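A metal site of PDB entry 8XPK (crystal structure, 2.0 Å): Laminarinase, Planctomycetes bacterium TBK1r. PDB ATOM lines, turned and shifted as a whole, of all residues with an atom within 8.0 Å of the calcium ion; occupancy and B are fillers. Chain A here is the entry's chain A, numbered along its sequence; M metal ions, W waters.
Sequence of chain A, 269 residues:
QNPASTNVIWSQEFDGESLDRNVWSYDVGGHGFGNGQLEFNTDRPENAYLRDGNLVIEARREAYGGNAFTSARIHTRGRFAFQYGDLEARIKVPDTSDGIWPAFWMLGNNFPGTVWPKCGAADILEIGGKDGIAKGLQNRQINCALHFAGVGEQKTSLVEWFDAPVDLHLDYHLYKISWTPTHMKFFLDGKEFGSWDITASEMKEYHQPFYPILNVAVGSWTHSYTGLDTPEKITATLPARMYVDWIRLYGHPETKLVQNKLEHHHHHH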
ATOM      1  N   GLN A  12     -12.258  17.544  29.960  1.00  0.00           N
ATOM      2  CA  GLN A  12     -12.061  18.914  30.357  1.00  0.00           C
ATOM      3  C   GLN A  12     -12.297  19.760  29.124  1.00  0.00           C
ATOM      4  O   GLN A  12     -11.604  19.594  28.124  1.00  0.00           O
ATOM      5  CB  GLN A  12     -10.644  19.050  30.914  1.00  0.00           C
ATOM      6  CG  GLN A  12     -10.431  18.462  32.302  1.00  0.00           C
ATOM      7  CD  GLN A  12     -11.053  19.319  33.382  1.00  0.00           C
ATOM      8  OE1 GLN A  12     -12.098  18.953  33.923  1.00  0.00           O
ATOM      9  NE2 GLN A  12     -10.486  20.481  33.655  1.00  0.00           N
ATOM     10  N   GLU A  13     -13.271  20.676  29.217  1.00  0.00           N
ATOM     11  CA  GLU A  13     -13.655  21.528  28.097  1.00  0.00           C
ATOM     12  C   GLU A  13     -13.005  22.907  28.185  1.00  0.00           C
ATOM     13  O   GLU A  13     -13.025  23.666  27.210  1.00  0.00           O
ATOM     14  CB  GLU A  13     -15.173  21.610  28.066  1.00  0.00           C
ATOM     15  CG  GLU A  13     -15.855  20.260  27.856  1.00  0.00           C
ATOM     16  CD  GLU A  13     -15.485  19.598  26.532  1.00  0.00           C
ATOM     17  OE1 GLU A  13     -15.306  20.308  25.506  1.00  0.00           O
ATOM     18  OE2 GLU A  13     -15.379  18.346  26.529  1.00  0.00           O
ATOM     19  N   PHE A  14     -12.448  23.225  29.365  1.00  0.00           N
ATOM     20  CA  PHE A  14     -11.652  24.417  29.603  1.00  0.00           C
ATOM     21  C   PHE A  14     -12.476  25.670  29.306  1.00  0.00           C
ATOM     22  O   PHE A  14     -11.960  26.625  28.715  1.00  0.00           O
ATOM     23  CB  PHE A  14     -10.365  24.474  28.782  1.00  0.00           C
ATOM     24  CG  PHE A  14      -9.455  23.286  29.009  1.00  0.00           C
ATOM     25  CD1 PHE A  14      -8.877  23.078  30.276  1.00  0.00           C
ATOM     26  CD2 PHE A  14      -9.196  22.377  28.000  1.00  0.00           C
ATOM     27  CE1 PHE A  14      -8.051  21.989  30.487  1.00  0.00           C
ATOM     28  CE2 PHE A  14      -8.338  21.296  28.208  1.00  0.00           C
ATOM     29  CZ  PHE A  14      -7.790  21.103  29.458  1.00  0.00           C
ATOM     30  N   ASP A  15     -13.743  25.618  29.696  1.00  0.00           N
ATOM     31  CA  ASP A  15     -14.649  26.744  29.656  1.00  0.00           C
ATOM     32  C   ASP A  15     -14.297  27.840  30.666  1.00  0.00           C
ATOM     33  O   ASP A  15     -14.520  28.999  30.369  1.00  0.00           O
ATOM     34  CB  ASP A  15     -16.058  26.306  30.015  1.00  0.00           C
ATOM     35  CG  ASP A  15     -16.174  25.445  31.271  1.00  0.00           C
ATOM     36  OD1 ASP A  15     -15.343  24.483  31.400  1.00  0.00           O
ATOM     37  OD2 ASP A  15     -17.073  25.733  32.101  1.00  0.00           O
ATOM     38  N   GLY A  16     -13.834  27.524  31.874  1.00  0.00           N
ATOM     39  CA  GLY A  16     -13.899  28.539  32.917  1.00  0.00           C
ATOM     40  C   GLY A  16     -12.983  29.760  32.670  1.00  0.00           C
ATOM     41  O   GLY A  16     -12.503  30.005  31.570  1.00  0.00           O
ATOM     42  N   ARG A  51      -8.988  30.993  28.708  1.00  0.00           N
ATOM     43  CA  ARG A  51      -9.858  32.064  28.229  1.00  0.00           C
ATOM     44  C   ARG A  51     -10.471  31.644  26.898  1.00  0.00           C
ATOM     45  O   ARG A  51      -9.869  30.888  26.158  1.00  0.00           O
ATOM     46  CB  ARG A  51      -9.155  33.426  28.151  1.00  0.00           C
ATOM     47  CG  ARG A  51      -8.073  33.509  27.094  1.00  0.00           C
ATOM     48  CD  ARG A  51      -7.178  34.716  27.285  1.00  0.00           C
ATOM     49  NE  ARG A  51      -6.151  34.825  26.238  1.00  0.00           N
ATOM     50  CZ  ARG A  51      -5.191  35.729  26.272  1.00  0.00           C
ATOM     51  NH1 ARG A  51      -5.061  36.471  27.358  1.00  0.00           N
ATOM     52  NH2 ARG A  51      -4.287  35.789  25.307  1.00  0.00           N
ATOM     53  N   ASP A  52     -11.685  32.119  26.661  1.00  0.00           N
ATOM     54  CA  ASP A  52     -12.372  31.937  25.382  1.00  0.00           C
ATOM     55  C   ASP A  52     -12.555  30.459  25.031  1.00  0.00           C
ATOM     56  O   ASP A  52     -12.677  30.142  23.852  1.00  0.00           O
ATOM     57  CB  ASP A  52     -11.669  32.719  24.293  1.00  0.00           C
ATOM     58  CG  ASP A  52     -11.545  34.207  24.587  1.00  0.00           C
ATOM     59  OD1 ASP A  52     -12.501  34.793  25.143  1.00  0.00           O
ATOM     60  OD2 ASP A  52     -10.515  34.778  24.189  1.00  0.00           O
ATOM     61  N   GLY A  53     -12.599  29.575  26.039  1.00  0.00           N
ATOM     62  CA  GLY A  53     -12.918  28.178  25.828  1.00  0.00           C
ATOM     63  C   GLY A  53     -11.657  27.310  25.651  1.00  0.00           C
ATOM     64  O   GLY A  53     -11.778  26.128  25.340  1.00  0.00           O
ATOM     65  N   ASN A  54     -10.477  27.913  25.866  1.00  0.00           N
ATOM     66  CA  ASN A  54      -9.222  27.191  25.703  1.00  0.00           C
ATOM     67  C   ASN A  54      -8.387  27.200  26.984  1.00  0.00           C
ATOM     68  O   ASN A  54      -8.296  28.221  27.671  1.00  0.00           O
ATOM     69  CB  ASN A  54      -8.309  27.812  24.666  1.00  0.00           C
ATOM     70  CG  ASN A  54      -8.886  27.787  23.271  1.00  0.00           C
ATOM     71  OD1 ASN A  54      -9.075  26.700  22.713  1.00  0.00           O
ATOM     72  ND2 ASN A  54      -9.050  28.950  22.666  1.00  0.00           N
ATOM     73  N   LEU A  55      -7.697  26.082  27.224  1.00  0.00           N
ATOM     74  CA  LEU A  55      -6.493  26.123  28.016  1.00  0.00           C
ATOM     75  C   LEU A  55      -5.415  26.769  27.146  1.00  0.00           C
ATOM     76  O   LEU A  55      -5.294  26.417  25.982  1.00  0.00           O
ATOM     77  CB  LEU A  55      -6.078  24.735  28.483  1.00  0.00           C
ATOM     78  CG  LEU A  55      -4.596  24.603  28.894  1.00  0.00           C
ATOM     79  CD1 LEU A  55      -4.377  25.244  30.240  1.00  0.00           C
ATOM     80  CD2 LEU A  55      -4.171  23.173  28.934  1.00  0.00           C
ATOM     81  N   ARG A  90      -8.078  18.449  21.221  1.00  0.00           N
ATOM     82  CA  ARG A  90      -8.127  19.396  20.123  1.00  0.00           C
ATOM     83  C   ARG A  90      -7.132  20.501  20.435  1.00  0.00           C
ATOM     84  O   ARG A  90      -7.340  21.264  21.375  1.00  0.00           O
ATOM     85  CB  ARG A  90      -9.568  19.884  19.939  1.00  0.00           C
ATOM     86  CG  ARG A  90      -9.682  20.865  18.767  1.00  0.00           C
ATOM     87  CD  ARG A  90     -11.110  21.157  18.406  1.00  0.00           C
ATOM     88  NE  ARG A  90     -11.201  21.857  17.113  1.00  0.00           N
ATOM     89  CZ  ARG A  90     -11.387  23.153  16.930  1.00  0.00           C
ATOM     90  NH1 ARG A  90     -11.455  23.972  17.963  1.00  0.00           N
ATOM     91  NH2 ARG A  90     -11.470  23.651  15.710  1.00  0.00           N
ATOM     92  N   TYR A 172      -6.359  24.291  14.758  1.00  0.00           N
ATOM     93  CA  TYR A 172      -6.584  23.198  15.693  1.00  0.00           C
ATOM     94  C   TYR A 172      -6.567  21.896  14.895  1.00  0.00           C
ATOM     95  O   TYR A 172      -7.069  21.830  13.780  1.00  0.00           O
ATOM     96  CB  TYR A 172      -7.949  23.331  16.405  1.00  0.00           C
ATOM     97  CG  TYR A 172      -8.043  24.503  17.365  1.00  0.00           C
ATOM     98  CD1 TYR A 172      -8.504  25.753  16.935  1.00  0.00           C
ATOM     99  CD2 TYR A 172      -7.729  24.351  18.714  1.00  0.00           C
ATOM    100  CE1 TYR A 172      -8.580  26.831  17.807  1.00  0.00           C
ATOM    101  CE2 TYR A 172      -7.786  25.425  19.583  1.00  0.00           C
ATOM    102  CZ  TYR A 172      -8.243  26.661  19.136  1.00  0.00           C
ATOM    103  OH  TYR A 172      -8.343  27.715  20.023  1.00  0.00           O
ATOM    104  N   VAL A 244      -5.488  24.521  23.892  1.00  0.00           N
ATOM    105  CA  VAL A 244      -6.170  23.240  23.989  1.00  0.00           C
ATOM    106  C   VAL A 244      -7.643  23.520  24.248  1.00  0.00           C
ATOM    107  O   VAL A 244      -7.997  24.019  25.298  1.00  0.00           O
ATOM    108  CB  VAL A 244      -5.640  22.319  25.091  1.00  0.00           C
ATOM    109  CG1 VAL A 244      -6.348  20.965  25.056  1.00  0.00           C
ATOM    110  CG2 VAL A 244      -4.128  22.179  25.025  1.00  0.00           C
ATOM    111  N   ASP A 245      -8.466  23.229  23.256  1.00  0.00           N
ATOM    112  CA  ASP A 245      -9.890  23.522  23.339  1.00  0.00           C
ATOM    113  C   ASP A 245     -10.561  22.497  24.244  1.00  0.00           C
ATOM    114  O   ASP A 245     -11.477  22.809  24.992  1.00  0.00           O
ATOM    115  CB  ASP A 245     -10.528  23.539  21.956  1.00  0.00           C
ATOM    116  CG  ASP A 245     -12.015  23.850  21.869  1.00  0.00           C
ATOM    117  OD1 ASP A 245     -12.626  24.287  22.882  1.00  0.00           O
ATOM    118  OD2 ASP A 245     -12.571  23.613  20.782  1.00  0.00           O
ATOM    119  N   TRP A 246     -10.114  21.251  24.161  1.00  0.00           N
ATOM    120  CA  TRP A 246     -10.684  20.214  24.988  1.00  0.00           C
ATOM    121  C   TRP A 246      -9.824  18.964  24.973  1.00  0.00           C
ATOM    122  O   TRP A 246      -9.081  18.746  24.041  1.00  0.00           O
ATOM    123  CB  TRP A 246     -12.121  19.885  24.588  1.00  0.00           C
ATOM    124  CG  TRP A 246     -12.394  19.641  23.127  1.00  0.00           C
ATOM    125  CD1 TRP A 246     -13.028  20.491  22.269  1.00  0.00           C
ATOM    126  CD2 TRP A 246     -12.177  18.422  22.368  1.00  0.00           C
ATOM    127  NE1 TRP A 246     -13.172  19.928  21.035  1.00  0.00           N
ATOM    128  CE2 TRP A 246     -12.673  18.648  21.071  1.00  0.00           C
ATOM    129  CE3 TRP A 246     -11.598  17.181  22.670  1.00  0.00           C
ATOM    130  CZ2 TRP A 246     -12.622  17.678  20.077  1.00  0.00           C
ATOM    131  CZ3 TRP A 246     -11.542  16.231  21.683  1.00  0.00           C
ATOM    132  CH2 TRP A 246     -12.085  16.459  20.414  1.00  0.00           C
ATOM    133  N   ILE A 247      -9.976  18.166  26.039  1.00  0.00           N
ATOM    134  CA  ILE A 247      -9.445  16.819  26.108  1.00  0.00           C
ATOM    135  C   ILE A 247     -10.578  15.918  26.577  1.00  0.00           C
ATOM    136  O   ILE A 247     -11.247  16.246  27.566  1.00  0.00           O
ATOM    137  CB  ILE A 247      -8.166  16.729  26.971  1.00  0.00           C
ATOM    138  CG1 ILE A 247      -7.668  15.283  27.108  1.00  0.00           C
ATOM    139  CG2 ILE A 247      -8.351  17.395  28.350  1.00  0.00           C
ATOM    140  CD1 ILE A 247      -6.321  15.179  27.825  1.00  0.00           C
ATOM    141  N   ARG A 248     -10.837  14.861  25.786  1.00  0.00           N
ATOM    142  CA  ARG A 248     -11.983  13.978  26.000  1.00  0.00           C
ATOM    143  C   ARG A 248     -11.570  12.501  26.030  1.00  0.00           C
ATOM    144  O   ARG A 248     -10.741  12.074  25.219  1.00  0.00           O
ATOM    145  CB  ARG A 248     -13.030  14.152  24.907  1.00  0.00           C
ATOM    146  CG  ARG A 248     -13.668  15.530  24.969  1.00  0.00           C
ATOM    147  CD  ARG A 248     -14.466  15.860  23.713  1.00  0.00           C
ATOM    148  NE  ARG A 248     -15.113  17.165  23.827  1.00  0.00           N
ATOM    149  CZ  ARG A 248     -15.606  17.841  22.785  1.00  0.00           C
ATOM    150  NH1 ARG A 248     -15.685  17.260  21.598  1.00  0.00           N
ATOM    151  NH2 ARG A 248     -15.996  19.097  22.961  1.00  0.00           N
HETATM  152 CA    CA M   1     -13.213  24.411  24.924  1.00  0.00          CA
HETATM  153  O   HOH W   1     -14.916  22.727  24.610  1.00  0.00           O
HETATM  154  O   HOH W   2     -14.595  25.801  23.602  1.00  0.00           O
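The calcium ion is bound by OD1 of Asp 245 (2.1 Å), O of Gly 53 (2.3 Å), O of Asp 245 (2.4 Å), water W2 (2.4 Å), O of Glu 13 (2.4 Å) and water W1 (2.4 Å).
The calcium ion has six donor atoms within binding distance.
OD2 of Asp 245 is in salt-bridge range of NH1 of Arg 90 (3.1 Å).
The side-chain carboxylate (OE1) of Glu 13 lies within salt-bridge range of the guanidinium group (NH2) of Arg 248.
The nearest printed residue that does not touch the calcium ion is Trp 246 (4.5 Å).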
